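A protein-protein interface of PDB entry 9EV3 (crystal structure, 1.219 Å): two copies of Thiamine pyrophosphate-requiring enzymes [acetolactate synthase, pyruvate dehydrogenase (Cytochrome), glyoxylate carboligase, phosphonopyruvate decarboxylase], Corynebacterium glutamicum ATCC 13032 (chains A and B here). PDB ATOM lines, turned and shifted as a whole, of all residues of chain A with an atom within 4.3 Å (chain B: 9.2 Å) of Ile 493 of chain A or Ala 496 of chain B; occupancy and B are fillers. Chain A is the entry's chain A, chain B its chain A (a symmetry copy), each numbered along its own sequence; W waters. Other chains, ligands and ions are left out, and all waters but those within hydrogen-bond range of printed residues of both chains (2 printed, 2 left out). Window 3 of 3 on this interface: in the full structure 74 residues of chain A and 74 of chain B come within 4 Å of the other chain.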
ATOM      1  N   LEU A 446      -5.371  30.518  -1.440  1.00  0.00           N
ATOM      2  CA  LEU A 446      -6.260  31.685  -1.690  1.00  0.00           C
ATOM      3  C   LEU A 446      -7.063  31.965  -0.407  1.00  0.00           C
ATOM      4  O   LEU A 446      -7.409  33.117  -0.135  1.00  0.00           O
ATOM      5  CB  LEU A 446      -7.257  31.344  -2.809  1.00  0.00           C
ATOM      6  CG  LEU A 446      -6.646  31.274  -4.212  1.00  0.00           C
ATOM      7  CD1 LEU A 446      -7.722  30.841  -5.250  1.00  0.00           C
ATOM      8  CD2 LEU A 446      -6.003  32.569  -4.626  1.00  0.00           C
ATOM      9  N   VAL A 488      -9.737  25.859 -16.333  1.00  0.00           N
ATOM     10  CA  VAL A 488     -10.221  26.193 -15.018  1.00  0.00           C
ATOM     11  C   VAL A 488     -10.483  27.689 -14.955  1.00  0.00           C
ATOM     12  O   VAL A 488      -9.701  28.481 -15.520  1.00  0.00           O
ATOM     13  CB  VAL A 488      -9.154  25.794 -13.988  1.00  0.00           C
ATOM     14  CG1 VAL A 488      -9.554  26.259 -12.576  1.00  0.00           C
ATOM     15  CG2 VAL A 488      -8.926  24.254 -14.038  1.00  0.00           C
ATOM     16  N   ASN A 489     -11.581  28.074 -14.292  1.00  0.00           N
ATOM     17  CA  ASN A 489     -11.881  29.491 -14.137  1.00  0.00           C
ATOM     18  C   ASN A 489     -11.438  29.923 -12.764  1.00  0.00           C
ATOM     19  O   ASN A 489     -12.182  29.831 -11.777  1.00  0.00           O
ATOM     20  CB  ASN A 489     -13.386  29.726 -14.379  1.00  0.00           C
ATOM     21  CG  ASN A 489     -13.686  31.192 -14.525  1.00  0.00           C
ATOM     22  OD1 ASN A 489     -13.088  32.003 -13.821  1.00  0.00           O
ATOM     23  ND2 ASN A 489     -14.633  31.576 -15.415  1.00  0.00           N
ATOM     24  N   PHE A 490     -10.187  30.413 -12.674  1.00  0.00           N
ATOM     25  CA  PHE A 490      -9.659  30.850 -11.383  1.00  0.00           C
ATOM     26  C   PHE A 490     -10.329  32.132 -10.913  1.00  0.00           C
ATOM     27  O   PHE A 490     -10.405  32.343  -9.705  1.00  0.00           O
ATOM     28  CB  PHE A 490      -8.129  31.038 -11.422  1.00  0.00           C
ATOM     29  CG  PHE A 490      -7.412  29.729 -11.592  1.00  0.00           C
ATOM     30  CD1 PHE A 490      -7.232  28.877 -10.511  1.00  0.00           C
ATOM     31  CD2 PHE A 490      -6.897  29.360 -12.822  1.00  0.00           C
ATOM     32  CE1 PHE A 490      -6.588  27.654 -10.682  1.00  0.00           C
ATOM     33  CE2 PHE A 490      -6.200  28.173 -12.973  1.00  0.00           C
ATOM     34  CZ  PHE A 490      -6.103  27.309 -11.921  1.00  0.00           C
ATOM     35  N   ALA A 491     -10.831  32.965 -11.824  1.00  0.00           N
ATOM     36  CA  ALA A 491     -11.528  34.184 -11.348  1.00  0.00           C
ATOM     37  C   ALA A 491     -12.782  33.804 -10.595  1.00  0.00           C
ATOM     38  O   ALA A 491     -13.070  34.388  -9.527  1.00  0.00           O
ATOM     39  CB  ALA A 491     -11.889  35.080 -12.528  1.00  0.00           C
ATOM     40  N   GLU A 492     -13.528  32.783 -11.071  1.00  0.00           N
ATOM     41  CA  GLU A 492     -14.733  32.380 -10.356  1.00  0.00           C
ATOM     42  C   GLU A 492     -14.386  31.654  -9.065  1.00  0.00           C
ATOM     43  O   GLU A 492     -15.087  31.837  -8.060  1.00  0.00           O
ATOM     44  CB  GLU A 492     -15.660  31.553 -11.256  1.00  0.00           C
ATOM     45  CG  GLU A 492     -16.169  32.402 -12.408  1.00  0.00           C
ATOM     46  CD  GLU A 492     -17.315  31.818 -13.207  1.00  0.00           C
ATOM     47  OE1 GLU A 492     -17.746  30.685 -12.895  1.00  0.00           O
ATOM     48  OE2 GLU A 492     -17.777  32.495 -14.154  1.00  0.00           O
ATOM     49  N   ILE A 493     -13.285  30.864  -9.049  1.00  0.00           N
ATOM     50  CA  ILE A 493     -12.901  30.212  -7.789  1.00  0.00           C
ATOM     51  C   ILE A 493     -12.497  31.276  -6.762  1.00  0.00           C
ATOM     52  O   ILE A 493     -12.925  31.233  -5.590  1.00  0.00           O
ATOM     53  CB  ILE A 493     -11.759  29.234  -8.086  1.00  0.00           C
ATOM     54  CG1 ILE A 493     -12.339  28.024  -8.830  1.00  0.00           C
ATOM     55  CG2 ILE A 493     -11.109  28.766  -6.755  1.00  0.00           C
ATOM     56  CD1 ILE A 493     -11.166  27.106  -9.366  1.00  0.00           C
ATOM     57  N   ALA A 494     -11.696  32.288  -7.192  1.00  0.00           N
ATOM     58  CA  ALA A 494     -11.303  33.359  -6.275  1.00  0.00           C
ATOM     59  C   ALA A 494     -12.502  34.125  -5.760  1.00  0.00           C
ATOM     60  O   ALA A 494     -12.572  34.417  -4.545  1.00  0.00           O
ATOM     61  CB  ALA A 494     -10.352  34.337  -6.977  1.00  0.00           C
ATOM     62  N   ALA A 495     -13.470  34.434  -6.618  1.00  0.00           N
ATOM     63  CA  ALA A 495     -14.655  35.151  -6.162  1.00  0.00           C
ATOM     64  C   ALA A 495     -15.443  34.298  -5.182  1.00  0.00           C
ATOM     65  O   ALA A 495     -15.966  34.843  -4.178  1.00  0.00           O
ATOM     66  CB  ALA A 495     -15.519  35.520  -7.363  1.00  0.00           C
ATOM     67  N   ALA A 496     -15.514  32.986  -5.395  1.00  0.00           N
ATOM     68  CA  ALA A 496     -16.201  32.132  -4.456  1.00  0.00           C
ATOM     69  C   ALA A 496     -15.480  32.093  -3.111  1.00  0.00           C
ATOM     70  O   ALA A 496     -16.128  31.893  -2.076  1.00  0.00           O
ATOM     71  CB  ALA A 496     -16.294  30.714  -5.039  1.00  0.00           C
ATOM     72  N   ALA A 497     -14.157  32.311  -3.114  1.00  0.00           N
ATOM     73  CA  ALA A 497     -13.373  32.406  -1.893  1.00  0.00           C
ATOM     74  C   ALA A 497     -13.432  33.829  -1.273  1.00  0.00           C
ATOM     75  O   ALA A 497     -12.776  34.054  -0.249  1.00  0.00           O
ATOM     76  CB  ALA A 497     -11.930  31.992  -2.168  1.00  0.00           C
ATOM     77  N   ARG B  47      -3.130  17.471  -9.112  1.00  0.00           N
ATOM     78  CA  ARG B  47      -2.618  18.842  -9.094  1.00  0.00           C
ATOM     79  C   ARG B  47      -1.378  18.978  -8.176  1.00  0.00           C
ATOM     80  O   ARG B  47      -0.614  19.929  -8.359  1.00  0.00           O
ATOM     81  CB  ARG B  47      -3.702  19.800  -8.582  1.00  0.00           C
ATOM     82  CG  ARG B  47      -4.368  20.685  -9.619  1.00  0.00           C
ATOM     83  CD  ARG B  47      -4.719  20.045 -10.902  1.00  0.00           C
ATOM     84  NE  ARG B  47      -5.175  21.049 -11.859  1.00  0.00           N
ATOM     85  CZ  ARG B  47      -5.976  20.787 -12.890  1.00  0.00           C
ATOM     86  NH1 ARG B  47      -6.341  21.762 -13.710  1.00  0.00           N
ATOM     87  NH2 ARG B  47      -6.487  19.551 -13.062  1.00  0.00           N
ATOM     88  N   LEU B 443      -6.828  21.790  -1.558  1.00  0.00           N
ATOM     89  CA  LEU B 443      -8.057  22.209  -2.220  1.00  0.00           C
ATOM     90  C   LEU B 443      -8.013  22.000  -3.720  1.00  0.00           C
ATOM     91  O   LEU B 443      -9.061  21.791  -4.343  1.00  0.00           O
ATOM     92  CB  LEU B 443      -8.284  23.702  -1.886  1.00  0.00           C
ATOM     93  CG  LEU B 443      -9.612  24.294  -2.371  1.00  0.00           C
ATOM     94  CD1 LEU B 443     -10.786  23.646  -1.614  1.00  0.00           C
ATOM     95  CD2 LEU B 443      -9.606  25.765  -2.149  1.00  0.00           C
ATOM     96  N   GLY B 444      -6.824  22.109  -4.302  1.00  0.00           N
ATOM     97  CA  GLY B 444      -6.681  21.964  -5.744  1.00  0.00           C
ATOM     98  C   GLY B 444      -7.076  20.595  -6.260  1.00  0.00           C
ATOM     99  O   GLY B 444      -7.293  20.417  -7.468  1.00  0.00           O
ATOM    100  N   LEU B 446      -9.833  19.327  -5.912  1.00  0.00           N
ATOM    101  CA  LEU B 446     -11.195  19.395  -6.506  1.00  0.00           C
ATOM    102  C   LEU B 446     -11.052  19.476  -8.036  1.00  0.00           C
ATOM    103  O   LEU B 446     -11.922  18.992  -8.764  1.00  0.00           O
ATOM    104  CB  LEU B 446     -11.905  20.671  -6.026  1.00  0.00           C
ATOM    105  CG  LEU B 446     -12.344  20.647  -4.559  1.00  0.00           C
ATOM    106  CD1 LEU B 446     -12.972  22.015  -4.160  1.00  0.00           C
ATOM    107  CD2 LEU B 446     -13.296  19.522  -4.261  1.00  0.00           C
ATOM    108  N   LEU B 447      -9.951  20.116  -8.532  1.00  0.00           N
ATOM    109  CA  LEU B 447      -9.762  20.178 -10.000  1.00  0.00           C
ATOM    110  C   LEU B 447      -9.496  18.797 -10.574  1.00  0.00           C
ATOM    111  O   LEU B 447      -9.871  18.512 -11.711  1.00  0.00           O
ATOM    112  CB  LEU B 447      -8.633  21.142 -10.347  1.00  0.00           C
ATOM    113  CG  LEU B 447      -8.781  22.562  -9.741  1.00  0.00           C
ATOM    114  CD1 LEU B 447      -7.572  23.436 -10.112  1.00  0.00           C
ATOM    115  CD2 LEU B 447     -10.106  23.226 -10.222  1.00  0.00           C
ATOM    116  N   LYS B 450     -12.861  16.966 -10.885  1.00  0.00           N
ATOM    117  CA  LYS B 450     -13.582  17.472 -12.068  1.00  0.00           C
ATOM    118  C   LYS B 450     -12.930  16.913 -13.328  1.00  0.00           C
ATOM    119  O   LYS B 450     -13.633  16.422 -14.230  1.00  0.00           O
ATOM    120  CB  LYS B 450     -13.479  19.020 -12.082  1.00  0.00           C
ATOM    121  CG  LYS B 450     -13.977  19.681 -13.387  1.00  0.00           C
ATOM    122  CD  LYS B 450     -15.415  19.527 -13.563  1.00  0.00           C
ATOM    123  CE  LYS B 450     -15.897  20.453 -14.681  1.00  0.00           C
ATOM    124  NZ  LYS B 450     -15.562  19.932 -16.031  1.00  0.00           N
ATOM    125  N   VAL B 488     -15.725  29.612   5.137  1.00  0.00           N
ATOM    126  CA  VAL B 488     -15.483  29.410   3.731  1.00  0.00           C
ATOM    127  C   VAL B 488     -16.690  28.720   3.117  1.00  0.00           C
ATOM    128  O   VAL B 488     -17.284  27.825   3.752  1.00  0.00           O
ATOM    129  CB  VAL B 488     -14.230  28.537   3.570  1.00  0.00           C
ATOM    130  CG1 VAL B 488     -14.005  28.168   2.093  1.00  0.00           C
ATOM    131  CG2 VAL B 488     -12.996  29.275   4.168  1.00  0.00           C
ATOM    132  N   ASN B 489     -17.065  29.142   1.903  1.00  0.00           N
ATOM    133  CA  ASN B 489     -18.179  28.501   1.217  1.00  0.00           C
ATOM    134  C   ASN B 489     -17.622  27.521   0.219  1.00  0.00           C
ATOM    135  O   ASN B 489     -17.327  27.859  -0.937  1.00  0.00           O
ATOM    136  CB  ASN B 489     -19.067  29.579   0.562  1.00  0.00           C
ATOM    137  CG  ASN B 489     -20.375  28.995   0.105  1.00  0.00           C
ATOM    138  OD1 ASN B 489     -20.394  27.866  -0.381  1.00  0.00           O
ATOM    139  ND2 ASN B 489     -21.497  29.745   0.219  1.00  0.00           N
ATOM    140  N   PHE B 490     -17.463  26.257   0.658  1.00  0.00           N
ATOM    141  CA  PHE B 490     -16.919  25.233  -0.232  1.00  0.00           C
ATOM    142  C   PHE B 490     -17.910  24.862  -1.325  1.00  0.00           C
ATOM    143  O   PHE B 490     -17.472  24.452  -2.397  1.00  0.00           O
ATOM    144  CB  PHE B 490     -16.489  23.970   0.541  1.00  0.00           C
ATOM    145  CG  PHE B 490     -15.304  24.236   1.425  1.00  0.00           C
ATOM    146  CD1 PHE B 490     -14.024  24.286   0.891  1.00  0.00           C
ATOM    147  CD2 PHE B 490     -15.463  24.410   2.788  1.00  0.00           C
ATOM    148  CE1 PHE B 490     -12.932  24.557   1.713  1.00  0.00           C
ATOM    149  CE2 PHE B 490     -14.368  24.613   3.611  1.00  0.00           C
ATOM    150  CZ  PHE B 490     -13.125  24.743   3.061  1.00  0.00           C
ATOM    151  N   ALA B 491     -19.212  25.019  -1.090  1.00  0.00           N
ATOM    152  CA  ALA B 491     -20.163  24.703  -2.183  1.00  0.00           C
ATOM    153  C   ALA B 491     -19.968  25.664  -3.333  1.00  0.00           C
ATOM    154  O   ALA B 491     -19.969  25.238  -4.509  1.00  0.00           O
ATOM    155  CB  ALA B 491     -21.598  24.792  -1.676  1.00  0.00           C
ATOM    156  N   GLU B 492     -19.728  26.962  -3.046  1.00  0.00           N
ATOM    157  CA  GLU B 492     -19.516  27.911  -4.134  1.00  0.00           C
ATOM    158  C   GLU B 492     -18.158  27.701  -4.786  1.00  0.00           C
ATOM    159  O   GLU B 492     -18.046  27.841  -6.012  1.00  0.00           O
ATOM    160  CB  GLU B 492     -19.715  29.353  -3.656  1.00  0.00           C
ATOM    161  CG  GLU B 492     -21.157  29.575  -3.236  1.00  0.00           C
ATOM    162  CD  GLU B 492     -21.573  31.016  -3.021  1.00  0.00           C
ATOM    163  OE1 GLU B 492     -20.715  31.915  -3.174  1.00  0.00           O
ATOM    164  OE2 GLU B 492     -22.760  31.243  -2.692  1.00  0.00           O
ATOM    165  N   ILE B 493     -17.122  27.318  -4.001  1.00  0.00           N
ATOM    166  CA  ILE B 493     -15.821  27.046  -4.630  1.00  0.00           C
ATOM    167  C   ILE B 493     -15.940  25.826  -5.550  1.00  0.00           C
ATOM    168  O   ILE B 493     -15.464  25.843  -6.704  1.00  0.00           O
ATOM    169  CB  ILE B 493     -14.789  26.832  -3.518  1.00  0.00           C
ATOM    170  CG1 ILE B 493     -14.480  28.191  -2.875  1.00  0.00           C
ATOM    171  CG2 ILE B 493     -13.488  26.231  -4.117  1.00  0.00           C
ATOM    172  CD1 ILE B 493     -13.605  27.985  -1.572  1.00  0.00           C
ATOM    173  N   ALA B 494     -16.623  24.749  -5.075  1.00  0.00           N
ATOM    174  CA  ALA B 494     -16.809  23.565  -5.915  1.00  0.00           C
ATOM    175  C   ALA B 494     -17.589  23.884  -7.172  1.00  0.00           C
ATOM    176  O   ALA B 494     -17.207  23.421  -8.270  1.00  0.00           O
ATOM    177  CB  ALA B 494     -17.550  22.472  -5.134  1.00  0.00           C
ATOM    178  N   ALA B 495     -18.646  24.686  -7.072  1.00  0.00           N
ATOM    179  CA  ALA B 495     -19.414  25.040  -8.260  1.00  0.00           C
ATOM    180  C   ALA B 495     -18.560  25.857  -9.216  1.00  0.00           C
ATOM    181  O   ALA B 495     -18.656  25.651 -10.451  1.00  0.00           O
ATOM    182  CB  ALA B 495     -20.655  25.825  -7.848  1.00  0.00           C
ATOM    183  N   ALA B 496     -17.701  26.737  -8.707  1.00  0.00           N
ATOM    184  CA  ALA B 496     -16.828  27.489  -9.577  1.00  0.00           C
ATOM    185  C   ALA B 496     -15.819  26.579 -10.274  1.00  0.00           C
ATOM    186  O   ALA B 496     -15.380  26.894 -11.387  1.00  0.00           O
ATOM    187  CB  ALA B 496     -16.088  28.552  -8.751  1.00  0.00           C
ATOM    188  N   ALA B 497     -15.473  25.446  -9.645  1.00  0.00           N
ATOM    189  CA  ALA B 497     -14.607  24.446 -10.248  1.00  0.00           C
ATOM    190  C   ALA B 497     -15.390  23.485 -11.183  1.00  0.00           C
ATOM    191  O   ALA B 497     -14.775  22.562 -11.731  1.00  0.00           O
ATOM    192  CB  ALA B 497     -13.876  23.667  -9.158  1.00  0.00           C
ATOM    193  N   GLY B 498     -16.685  23.682 -11.354  1.00  0.00           N
ATOM    194  CA  GLY B 498     -17.443  22.835 -12.269  1.00  0.00           C
ATOM    195  C   GLY B 498     -17.955  21.558 -11.632  1.00  0.00           C
ATOM    196  O   GLY B 498     -18.328  20.601 -12.350  1.00  0.00           O
ATOM    197  N   ILE B 499     -18.050  21.530 -10.287  1.00  0.00           N
ATOM    198  CA  ILE B 499     -18.595  20.365  -9.582  1.00  0.00           C
ATOM    199  C   ILE B 499     -19.959  20.688  -9.025  1.00  0.00           C
ATOM    200  O   ILE B 499     -20.169  21.700  -8.337  1.00  0.00           O
ATOM    201  CB  ILE B 499     -17.615  19.935  -8.434  1.00  0.00           C
ATOM    202  CG1 ILE B 499     -16.254  19.562  -9.056  1.00  0.00           C
ATOM    203  CG2 ILE B 499     -18.162  18.729  -7.634  1.00  0.00           C
ATOM    204  CD1 ILE B 499     -15.154  19.460  -7.972  1.00  0.00           C
ATOM    205  N   LYS B 500     -20.897  19.757  -9.206  1.00  0.00           N
ATOM    206  CA  LYS B 500     -22.222  19.874  -8.588  1.00  0.00           C
ATOM    207  C   LYS B 500     -22.081  20.018  -7.076  1.00  0.00           C
ATOM    208  O   LYS B 500     -21.270  19.277  -6.480  1.00  0.00           O
ATOM    209  CB  LYS B 500     -23.007  18.584  -8.886  1.00  0.00           C
ATOM    210  CG  LYS B 500     -24.412  18.483  -8.267  1.00  0.00           C
ATOM    211  CD  LYS B 500     -25.381  19.411  -8.911  1.00  0.00           C
ATOM    212  CE  LYS B 500     -26.670  19.277  -8.130  1.00  0.00           C
ATOM    213  NZ  LYS B 500     -27.687  20.220  -8.673  1.00  0.00           N
ATOM    214  N   SER B 501     -22.767  20.957  -6.472  1.00  0.00           N
ATOM    215  CA  SER B 501     -22.649  21.136  -5.035  1.00  0.00           C
ATOM    216  C   SER B 501     -23.934  21.562  -4.367  1.00  0.00           C
ATOM    217  O   SER B 501     -24.894  22.008  -5.031  1.00  0.00           O
ATOM    218  CB  SER B 501     -21.549  22.142  -4.727  1.00  0.00           C
ATOM    219  OG  SER B 501     -22.002  23.428  -5.125  1.00  0.00           O
HETATM  220  O   HOH W   1     -15.800  31.339   0.656  1.00  0.00           O
HETATM  221  O   HOH W   2     -13.410  26.188 -13.258  1.00  0.00           O
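OD1 of Asn 489 of chain A sits at hydrogen-bond distance from N of Glu 492 of chain A, 2.9 Å away. OD1 of Asn 489 of chain B sits at hydrogen-bond distance from N of Glu 492 of chain B (2.9 Å).
Val 488 of chain A touches Arg 47 of chain B (CG2 to NH1, 3.6 Å). Leu 447 of chain B touches Val 488 of chain A (CD2 to CG1, 3.9 Å). Glu 492 of chain A touches Ala 496 of chain B. Ile 493 of chain A touches Ala 496 of chain B (N to CB, 3.6 Å). Ala 496 of chain A touches Glu 492 of chain B (CB to O, 3.5 Å). CB of Ala 496 of chain A touches N of Ile 493 of chain B (3.6 Å).
Of chain B, only Ala 496 comes within 4 Å of Ile 493 of chain A. Printed residues of chain B within 4 Å of Ala 496 of chain A: Glu 492 (3.5 Å) and Ile 493 (3.6 Å). Printed residues of chain A within 4 Å of Glu 492 of chain B: Ala 496 (3.5 Å). Of the printed residues of chain B, Glu 492 of chain A touches Ala 496. Of the printed residues of chain A, Leu 447 of chain B touches Val 488 (3.9 Å). Ala 495 of chain A touches none of the printed residues of chain B. Leu 446 of chain B touches none of the printed residues of chain A. The nearest printed residue of chain B that does not touch Ile 493 of chain A is Leu 447 of chain B (4.1 Å). The nearest printed residue of chain A that does not touch Ala 496 of chain B is Ala 496 of chain A (4.3 Å).
Hydrophobic or aromatic side chains of chain A that line the printed part of chain B: Val 488, Ile 493 and Ala 496. Among the printed residues, no Asp or Glu carboxylate lies within 4 Å of a Lys or Arg side-chain nitrogen of the other chain.
Glu 492 of chain A touches Ala 496 of chain B, and with the chains exchanged Ala 496 of chain A touches Glu 492 of chain B. Ile 493 of chain A touches Ala 496 of chain B, and with the chains exchanged Ala 496 of chain A touches Ile 493 of chain B. Of the 6 pairs that touch across the chains among the printed residues, 4 have their exchanged pair printed and touching as well.
Water W1 lies within hydrogen-bond range of O of Ala 496 of chain A (2.8 Å) and N of Asn 489 of chain B (2.8 Å). Water W2 bridges O of Ala 496 of chain B (2.8 Å) and N of Asn 489 of chain A (2.8 Å).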
